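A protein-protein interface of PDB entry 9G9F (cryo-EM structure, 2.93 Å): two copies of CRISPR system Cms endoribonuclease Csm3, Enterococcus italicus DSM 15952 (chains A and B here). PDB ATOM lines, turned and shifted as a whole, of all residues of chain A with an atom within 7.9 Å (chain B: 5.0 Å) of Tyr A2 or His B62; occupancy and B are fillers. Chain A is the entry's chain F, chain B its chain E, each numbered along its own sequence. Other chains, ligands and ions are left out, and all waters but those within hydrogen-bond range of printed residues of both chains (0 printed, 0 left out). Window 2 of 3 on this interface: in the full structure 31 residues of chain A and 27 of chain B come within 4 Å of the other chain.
NE2 of Gln A97 sits at hydrogen-bond distance from OD1 of Asp B179 (2.9 Å).
NZ of Lys A4 is in hydrogen-bond range of O of Leu B175, 3.4 Å away.
NE2 of Gln A97 sits at hydrogen-bond distance from OD1 of Asn A155 (3.2 Å).
O of Lys A4 lies within hydrogen-bond range of N of Val A202, at 3.1 Å.
OH of Tyr A2 lies within hydrogen-bond range of NZ of Lys A4, at 2.9 Å.
The backbone NH (N) of Gln A97 sits at hydrogen-bond distance from the backbone carbonyl oxygen (O) of Ile A153 (3.2 Å).
N of Lys A4 lies within hydrogen-bond range of O of Val A203, 2.9 Å away.
Tyr A2 touches Leu B58.
Tyr A2 touches Lys B61.
CB of Tyr A2 touches CA of His B62 (3.5 Å).
CE2 of Tyr A2 touches CD2 of Leu B175 (3.5 Å).
Leu B58 touches Lys A4 (CD2 to NZ, 3.8 Å).
Lys A4 touches Asp B179 (CE to CB, 3.8 Å).
CD2 of Leu B175 touches CG1 of Val A203 (3.6 Å).
Tyr A2 touches just these residues of chain B: Leu B58 (3.2 Å), Lys B61 (3.5 Å), His B62 (3.5 Å) and Leu B175 (3.5 Å).
His B62 touches one residue of chain A.
Of the printed residues of chain A, Asp B179 touches Lys A4 (3.8 Å) and Gln A97 (2.9 Å).
Printed residues of chain A within 4 Å of Lys B61: Tyr A2.
Ile B63 touches none of the printed residues of chain A.
Phe A206 touches none of the printed residues of chain B.
The nearest printed residue of chain B that does not touch Lys A4 is Thr B171 (7.0 Å).
Of the 10 printed residues of chain B, 5 touch a printed residue of chain A.
Of the 17 printed residues of chain A, 4 touch a printed residue of chain B.
Among the printed residues, 9 pairs touch across the chains.
Among the printed residues, no Asp or Glu carboxylate lies within 4 Å of a Lys or Arg side-chain nitrogen of the other chain.
No position is printed for both chains.
Of the 9 pairs that touch across the chains among the printed residues, none has its exchanged pair printed and touching as well.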
ATOM      1  N   TYR A   2      -0.961  -2.922 -25.522  1.00  0.00           N
ATOM      2  CA  TYR A   2      -1.766  -4.095 -25.208  1.00  0.00           C
ATOM      3  C   TYR A   2      -2.272  -4.769 -26.474  1.00  0.00           C
ATOM      4  O   TYR A   2      -3.354  -4.453 -26.967  1.00  0.00           O
ATOM      5  CB  TYR A   2      -2.940  -3.713 -24.314  1.00  0.00           C
ATOM      6  CG  TYR A   2      -3.839  -4.867 -23.941  1.00  0.00           C
ATOM      7  CD1 TYR A   2      -3.339  -5.977 -23.279  1.00  0.00           C
ATOM      8  CD2 TYR A   2      -5.194  -4.837 -24.236  1.00  0.00           C
ATOM      9  CE1 TYR A   2      -4.159  -7.027 -22.932  1.00  0.00           C
ATOM     10  CE2 TYR A   2      -6.021  -5.882 -23.891  1.00  0.00           C
ATOM     11  CZ  TYR A   2      -5.498  -6.974 -23.240  1.00  0.00           C
ATOM     12  OH  TYR A   2      -6.318  -8.019 -22.894  1.00  0.00           O
ATOM     13  N   SER A   3      -1.479  -5.701 -26.992  1.00  0.00           N
ATOM     14  CA  SER A   3      -1.794  -6.430 -28.210  1.00  0.00           C
ATOM     15  C   SER A   3      -2.046  -7.894 -27.883  1.00  0.00           C
ATOM     16  O   SER A   3      -1.369  -8.475 -27.028  1.00  0.00           O
ATOM     17  CB  SER A   3      -0.659  -6.316 -29.230  1.00  0.00           C
ATOM     18  OG  SER A   3      -0.364  -4.964 -29.526  1.00  0.00           O
ATOM     19  N   LYS A   4      -3.024  -8.483 -28.566  1.00  0.00           N
ATOM     20  CA  LYS A   4      -3.333  -9.900 -28.444  1.00  0.00           C
ATOM     21  C   LYS A   4      -2.839 -10.621 -29.690  1.00  0.00           C
ATOM     22  O   LYS A   4      -3.255 -10.294 -30.805  1.00  0.00           O
ATOM     23  CB  LYS A   4      -4.836 -10.116 -28.264  1.00  0.00           C
ATOM     24  CG  LYS A   4      -5.392  -9.622 -26.943  1.00  0.00           C
ATOM     25  CD  LYS A   4      -6.617 -10.426 -26.554  1.00  0.00           C
ATOM     26  CE  LYS A   4      -7.176 -10.009 -25.207  1.00  0.00           C
ATOM     27  NZ  LYS A   4      -7.813  -8.669 -25.266  1.00  0.00           N
ATOM     28  N   ILE A   5      -1.958 -11.597 -29.504  1.00  0.00           N
ATOM     29  CA  ILE A   5      -1.413 -12.379 -30.605  1.00  0.00           C
ATOM     30  C   ILE A   5      -2.138 -13.716 -30.642  1.00  0.00           C
ATOM     31  O   ILE A   5      -2.129 -14.465 -29.658  1.00  0.00           O
ATOM     32  CB  ILE A   5       0.103 -12.570 -30.465  1.00  0.00           C
ATOM     33  CG1 ILE A   5       0.819 -11.229 -30.627  1.00  0.00           C
ATOM     34  CG2 ILE A   5       0.611 -13.564 -31.487  1.00  0.00           C
ATOM     35  CD1 ILE A   5       2.324 -11.345 -30.674  1.00  0.00           C
ATOM     36  N   GLN A  97      -4.387 -18.432 -23.180  1.00  0.00           N
ATOM     37  CA  GLN A  97      -5.781 -18.855 -23.066  1.00  0.00           C
ATOM     38  C   GLN A  97      -6.074 -19.855 -24.180  1.00  0.00           C
ATOM     39  O   GLN A  97      -6.574 -19.490 -25.244  1.00  0.00           O
ATOM     40  CB  GLN A  97      -6.700 -17.649 -23.140  1.00  0.00           C
ATOM     41  CG  GLN A  97      -6.244 -16.481 -22.292  1.00  0.00           C
ATOM     42  CD  GLN A  97      -7.129 -15.268 -22.454  1.00  0.00           C
ATOM     43  OE1 GLN A  97      -8.125 -15.308 -23.170  1.00  0.00           O
ATOM     44  NE2 GLN A  97      -6.770 -14.179 -21.788  1.00  0.00           N
ATOM     45  N   ILE A 153      -4.772 -17.630 -27.600  1.00  0.00           N
ATOM     46  CA  ILE A 153      -4.573 -16.187 -27.612  1.00  0.00           C
ATOM     47  C   ILE A 153      -3.598 -15.822 -26.505  1.00  0.00           C
ATOM     48  O   ILE A 153      -3.780 -16.226 -25.353  1.00  0.00           O
ATOM     49  CB  ILE A 153      -5.900 -15.424 -27.457  1.00  0.00           C
ATOM     50  CG1 ILE A 153      -6.536 -15.243 -28.831  1.00  0.00           C
ATOM     51  CG2 ILE A 153      -5.681 -14.086 -26.783  1.00  0.00           C
ATOM     52  CD1 ILE A 153      -8.006 -15.037 -28.800  1.00  0.00           C
ATOM     53  N   TYR A 154      -2.558 -15.072 -26.857  1.00  0.00           N
ATOM     54  CA  TYR A 154      -1.520 -14.665 -25.923  1.00  0.00           C
ATOM     55  C   TYR A 154      -1.575 -13.156 -25.758  1.00  0.00           C
ATOM     56  O   TYR A 154      -1.498 -12.416 -26.745  1.00  0.00           O
ATOM     57  CB  TYR A 154      -0.140 -15.109 -26.415  1.00  0.00           C
ATOM     58  CG  TYR A 154       1.000 -14.674 -25.528  1.00  0.00           C
ATOM     59  CD1 TYR A 154       1.444 -15.475 -24.488  1.00  0.00           C
ATOM     60  CD2 TYR A 154       1.639 -13.464 -25.738  1.00  0.00           C
ATOM     61  CE1 TYR A 154       2.485 -15.074 -23.680  1.00  0.00           C
ATOM     62  CE2 TYR A 154       2.676 -13.059 -24.939  1.00  0.00           C
ATOM     63  CZ  TYR A 154       3.096 -13.865 -23.913  1.00  0.00           C
ATOM     64  OH  TYR A 154       4.135 -13.443 -23.123  1.00  0.00           O
ATOM     65  N   ASN A 155      -1.702 -12.703 -24.517  1.00  0.00           N
ATOM     66  CA  ASN A 155      -1.663 -11.280 -24.226  1.00  0.00           C
ATOM     67  C   ASN A 155      -0.227 -10.842 -23.984  1.00  0.00           C
ATOM     68  O   ASN A 155       0.500 -11.452 -23.196  1.00  0.00           O
ATOM     69  CB  ASN A 155      -2.524 -10.963 -23.005  1.00  0.00           C
ATOM     70  CG  ASN A 155      -3.851 -11.683 -23.028  1.00  0.00           C
ATOM     71  OD1 ASN A 155      -4.252 -12.298 -22.043  1.00  0.00           O
ATOM     72  ND2 ASN A 155      -4.543 -11.611 -24.156  1.00  0.00           N
ATOM     73  N   VAL A 156       0.185  -9.785 -24.673  1.00  0.00           N
ATOM     74  CA  VAL A 156       1.550  -9.280 -24.588  1.00  0.00           C
ATOM     75  C   VAL A 156       1.577  -8.235 -23.479  1.00  0.00           C
ATOM     76  O   VAL A 156       1.260  -7.065 -23.705  1.00  0.00           O
ATOM     77  CB  VAL A 156       2.025  -8.705 -25.922  1.00  0.00           C
ATOM     78  CG1 VAL A 156       3.467  -8.244 -25.808  1.00  0.00           C
ATOM     79  CG2 VAL A 156       1.863  -9.733 -27.023  1.00  0.00           C
ATOM     80  N   GLU A 157       1.952  -8.654 -22.273  1.00  0.00           N
ATOM     81  CA  GLU A 157       2.042  -7.745 -21.137  1.00  0.00           C
ATOM     82  C   GLU A 157       3.464  -7.261 -20.891  1.00  0.00           C
ATOM     83  O   GLU A 157       3.692  -6.059 -20.743  1.00  0.00           O
ATOM     84  CB  GLU A 157       1.489  -8.418 -19.874  1.00  0.00           C
ATOM     85  CG  GLU A 157      -0.025  -8.671 -19.852  1.00  0.00           C
ATOM     86  CD  GLU A 157      -0.865  -7.607 -20.551  1.00  0.00           C
ATOM     87  OE1 GLU A 157      -1.933  -7.972 -21.081  1.00  0.00           O
ATOM     88  OE2 GLU A 157      -0.510  -6.409 -20.516  1.00  0.00           O
ATOM     89  N   ILE A 159       6.650  -6.865 -22.807  1.00  0.00           N
ATOM     90  CA  ILE A 159       7.106  -6.899 -24.193  1.00  0.00           C
ATOM     91  C   ILE A 159       8.512  -7.480 -24.280  1.00  0.00           C
ATOM     92  O   ILE A 159       8.854  -8.177 -25.243  1.00  0.00           O
ATOM     93  CB  ILE A 159       7.023  -5.489 -24.810  1.00  0.00           C
ATOM     94  CG1 ILE A 159       5.577  -5.152 -25.179  1.00  0.00           C
ATOM     95  CG2 ILE A 159       7.913  -5.368 -26.037  1.00  0.00           C
ATOM     96  CD1 ILE A 159       4.778  -4.540 -24.052  1.00  0.00           C
ATOM     97  N   THR A 201      -1.301 -10.640 -35.118  1.00  0.00           N
ATOM     98  CA  THR A 201      -1.652  -9.723 -34.034  1.00  0.00           C
ATOM     99  C   THR A 201      -3.031  -9.150 -34.337  1.00  0.00           C
ATOM    100  O   THR A 201      -3.157  -8.190 -35.102  1.00  0.00           O
ATOM    101  CB  THR A 201      -0.610  -8.619 -33.892  1.00  0.00           C
ATOM    102  OG1 THR A 201       0.668  -9.205 -33.617  1.00  0.00           O
ATOM    103  CG2 THR A 201      -0.982  -7.685 -32.758  1.00  0.00           C
ATOM    104  N   VAL A 202      -4.065  -9.743 -33.739  1.00  0.00           N
ATOM    105  CA  VAL A 202      -5.433  -9.348 -34.058  1.00  0.00           C
ATOM    106  C   VAL A 202      -5.715  -7.934 -33.569  1.00  0.00           C
ATOM    107  O   VAL A 202      -6.235  -7.096 -34.314  1.00  0.00           O
ATOM    108  CB  VAL A 202      -6.431 -10.359 -33.470  1.00  0.00           C
ATOM    109  CG1 VAL A 202      -7.849  -9.865 -33.660  1.00  0.00           C
ATOM    110  CG2 VAL A 202      -6.250 -11.711 -34.124  1.00  0.00           C
ATOM    111  N   VAL A 203      -5.379  -7.643 -32.315  1.00  0.00           N
ATOM    112  CA  VAL A 203      -5.633  -6.339 -31.713  1.00  0.00           C
ATOM    113  C   VAL A 203      -4.311  -5.765 -31.226  1.00  0.00           C
ATOM    114  O   VAL A 203      -3.536  -6.459 -30.560  1.00  0.00           O
ATOM    115  CB  VAL A 203      -6.642  -6.428 -30.553  1.00  0.00           C
ATOM    116  CG1 VAL A 203      -7.171  -5.046 -30.212  1.00  0.00           C
ATOM    117  CG2 VAL A 203      -7.780  -7.356 -30.911  1.00  0.00           C
ATOM    118  N   GLY A 204      -4.059  -4.509 -31.556  1.00  0.00           N
ATOM    119  CA  GLY A 204      -2.864  -3.824 -31.112  1.00  0.00           C
ATOM    120  C   GLY A 204      -1.922  -3.519 -32.262  1.00  0.00           C
ATOM    121  O   GLY A 204      -2.269  -3.623 -33.442  1.00  0.00           O
ATOM    122  N   ASP A 205      -0.700  -3.131 -31.892  1.00  0.00           N
ATOM    123  CA  ASP A 205       0.312  -2.710 -32.852  1.00  0.00           C
ATOM    124  C   ASP A 205       1.612  -3.495 -32.707  1.00  0.00           C
ATOM    125  O   ASP A 205       2.667  -3.020 -33.136  1.00  0.00           O
ATOM    126  CB  ASP A 205       0.591  -1.210 -32.725  1.00  0.00           C
ATOM    127  CG  ASP A 205       1.073  -0.811 -31.339  1.00  0.00           C
ATOM    128  OD1 ASP A 205       0.519  -1.299 -30.331  1.00  0.00           O
ATOM    129  OD2 ASP A 205       2.019  -0.001 -31.257  1.00  0.00           O
ATOM    130  N   PHE A 206       1.562  -4.679 -32.105  1.00  0.00           N
ATOM    131  CA  PHE A 206       2.752  -5.506 -32.004  1.00  0.00           C
ATOM    132  C   PHE A 206       3.095  -6.106 -33.364  1.00  0.00           C
ATOM    133  O   PHE A 206       2.245  -6.233 -34.250  1.00  0.00           O
ATOM    134  CB  PHE A 206       2.546  -6.615 -30.973  1.00  0.00           C
ATOM    135  CG  PHE A 206       3.810  -7.069 -30.305  1.00  0.00           C
ATOM    136  CD1 PHE A 206       4.269  -6.435 -29.167  1.00  0.00           C
ATOM    137  CD2 PHE A 206       4.532  -8.136 -30.808  1.00  0.00           C
ATOM    138  CE1 PHE A 206       5.425  -6.851 -28.545  1.00  0.00           C
ATOM    139  CE2 PHE A 206       5.690  -8.556 -30.191  1.00  0.00           C
ATOM    140  CZ  PHE A 206       6.137  -7.912 -29.059  1.00  0.00           C
ATOM    141  N   LEU B  58     -10.461  -4.963 -19.796  1.00  0.00           N
ATOM    142  CA  LEU B  58      -9.731  -5.025 -21.058  1.00  0.00           C
ATOM    143  C   LEU B  58      -9.444  -3.633 -21.604  1.00  0.00           C
ATOM    144  O   LEU B  58      -8.336  -3.366 -22.084  1.00  0.00           O
ATOM    145  CB  LEU B  58     -10.514  -5.851 -22.073  1.00  0.00           C
ATOM    146  CG  LEU B  58     -10.679  -7.319 -21.696  1.00  0.00           C
ATOM    147  CD1 LEU B  58     -11.744  -7.964 -22.553  1.00  0.00           C
ATOM    148  CD2 LEU B  58      -9.361  -8.052 -21.827  1.00  0.00           C
ATOM    149  N   LEU B  59     -10.424  -2.729 -21.539  1.00  0.00           N
ATOM    150  CA  LEU B  59     -10.207  -1.378 -22.038  1.00  0.00           C
ATOM    151  C   LEU B  59      -9.167  -0.647 -21.203  1.00  0.00           C
ATOM    152  O   LEU B  59      -8.357   0.114 -21.742  1.00  0.00           O
ATOM    153  CB  LEU B  59     -11.528  -0.612 -22.058  1.00  0.00           C
ATOM    154  CG  LEU B  59     -11.594   0.654 -22.909  1.00  0.00           C
ATOM    155  CD1 LEU B  59     -10.975   0.422 -24.270  1.00  0.00           C
ATOM    156  CD2 LEU B  59     -13.033   1.095 -23.056  1.00  0.00           C
ATOM    157  N   ALA B  60      -9.170  -0.861 -19.886  1.00  0.00           N
ATOM    158  CA  ALA B  60      -8.153  -0.255 -19.039  1.00  0.00           C
ATOM    159  C   ALA B  60      -6.773  -0.810 -19.350  1.00  0.00           C
ATOM    160  O   ALA B  60      -5.787  -0.068 -19.336  1.00  0.00           O
ATOM    161  CB  ALA B  60      -8.499  -0.465 -17.568  1.00  0.00           C
ATOM    162  N   LYS B  61      -6.673  -2.113 -19.619  1.00  0.00           N
ATOM    163  CA  LYS B  61      -5.379  -2.676 -19.994  1.00  0.00           C
ATOM    164  C   LYS B  61      -4.892  -2.105 -21.321  1.00  0.00           C
ATOM    165  O   LYS B  61      -3.696  -1.841 -21.491  1.00  0.00           O
ATOM    166  CB  LYS B  61      -5.462  -4.200 -20.065  1.00  0.00           C
ATOM    167  CG  LYS B  61      -5.021  -4.901 -18.795  1.00  0.00           C
ATOM    168  CD  LYS B  61      -3.595  -4.528 -18.434  1.00  0.00           C
ATOM    169  CE  LYS B  61      -3.187  -5.143 -17.108  1.00  0.00           C
ATOM    170  NZ  LYS B  61      -4.027  -4.641 -15.987  1.00  0.00           N
ATOM    171  N   HIS B  62      -5.805  -1.916 -22.275  1.00  0.00           N
ATOM    172  CA  HIS B  62      -5.419  -1.372 -23.573  1.00  0.00           C
ATOM    173  C   HIS B  62      -4.981   0.082 -23.456  1.00  0.00           C
ATOM    174  O   HIS B  62      -3.949   0.477 -24.009  1.00  0.00           O
ATOM    175  CB  HIS B  62      -6.573  -1.508 -24.563  1.00  0.00           C
ATOM    176  CG  HIS B  62      -6.432  -0.646 -25.777  1.00  0.00           C
ATOM    177  ND1 HIS B  62      -7.391   0.267 -26.156  1.00  0.00           N
ATOM    178  CD2 HIS B  62      -5.442  -0.555 -26.696  1.00  0.00           C
ATOM    179  CE1 HIS B  62      -7.000   0.882 -27.257  1.00  0.00           C
ATOM    180  NE2 HIS B  62      -5.820   0.403 -27.605  1.00  0.00           N
ATOM    181  N   ILE B  63      -5.762   0.897 -22.746  1.00  0.00           N
ATOM    182  CA  ILE B  63      -5.426   2.308 -22.592  1.00  0.00           C
ATOM    183  C   ILE B  63      -4.183   2.469 -21.725  1.00  0.00           C
ATOM    184  O   ILE B  63      -3.327   3.319 -21.995  1.00  0.00           O
ATOM    185  CB  ILE B  63      -6.627   3.077 -22.019  1.00  0.00           C
ATOM    186  CG1 ILE B  63      -7.792   3.031 -23.002  1.00  0.00           C
ATOM    187  CG2 ILE B  63      -6.251   4.511 -21.739  1.00  0.00           C
ATOM    188  CD1 ILE B  63      -7.487   3.685 -24.323  1.00  0.00           C
ATOM    189  N   GLY B  64      -4.062   1.657 -20.683  1.00  0.00           N
ATOM    190  CA  GLY B  64      -2.922   1.725 -19.793  1.00  0.00           C
ATOM    191  C   GLY B  64      -3.331   2.016 -18.368  1.00  0.00           C
ATOM    192  O   GLY B  64      -4.150   2.905 -18.120  1.00  0.00           O
ATOM    193  N   THR B 171     -13.353  -0.757 -29.471  1.00  0.00           N
ATOM    194  CA  THR B 171     -12.087  -1.370 -29.089  1.00  0.00           C
ATOM    195  C   THR B 171     -12.290  -2.387 -27.978  1.00  0.00           C
ATOM    196  O   THR B 171     -11.711  -3.476 -28.002  1.00  0.00           O
ATOM    197  CB  THR B 171     -11.090  -0.294 -28.659  1.00  0.00           C
ATOM    198  OG1 THR B 171     -10.628   0.418 -29.812  1.00  0.00           O
ATOM    199  CG2 THR B 171      -9.903  -0.919 -27.948  1.00  0.00           C
ATOM    200  N   LEU B 175     -11.648  -6.358 -28.091  1.00  0.00           N
ATOM    201  CA  LEU B 175     -10.842  -7.020 -27.074  1.00  0.00           C
ATOM    202  C   LEU B 175     -11.606  -8.167 -26.432  1.00  0.00           C
ATOM    203  O   LEU B 175     -11.020  -9.201 -26.107  1.00  0.00           O
ATOM    204  CB  LEU B 175     -10.407  -6.010 -26.015  1.00  0.00           C
ATOM    205  CG  LEU B 175      -9.349  -4.984 -26.416  1.00  0.00           C
ATOM    206  CD1 LEU B 175      -9.128  -3.995 -25.292  1.00  0.00           C
ATOM    207  CD2 LEU B 175      -8.055  -5.671 -26.778  1.00  0.00           C
ATOM    208  N   ASP B 179     -10.698 -11.800 -25.919  1.00  0.00           N
ATOM    209  CA  ASP B 179     -10.693 -12.263 -24.498  1.00  0.00           C
ATOM    210  C   ASP B 179     -11.967 -13.050 -24.167  1.00  0.00           C
ATOM    211  O   ASP B 179     -12.860 -13.126 -25.006  1.00  0.00           O
ATOM    212  CB  ASP B 179     -10.446 -11.117 -23.534  1.00  0.00           C
ATOM    213  CG  ASP B 179      -9.962 -11.540 -22.156  1.00  0.00           C
ATOM    214  OD1 ASP B 179      -8.882 -12.164 -22.080  1.00  0.00           O
ATOM    215  OD2 ASP B 179     -10.676 -11.255 -21.180  1.00  0.00           O
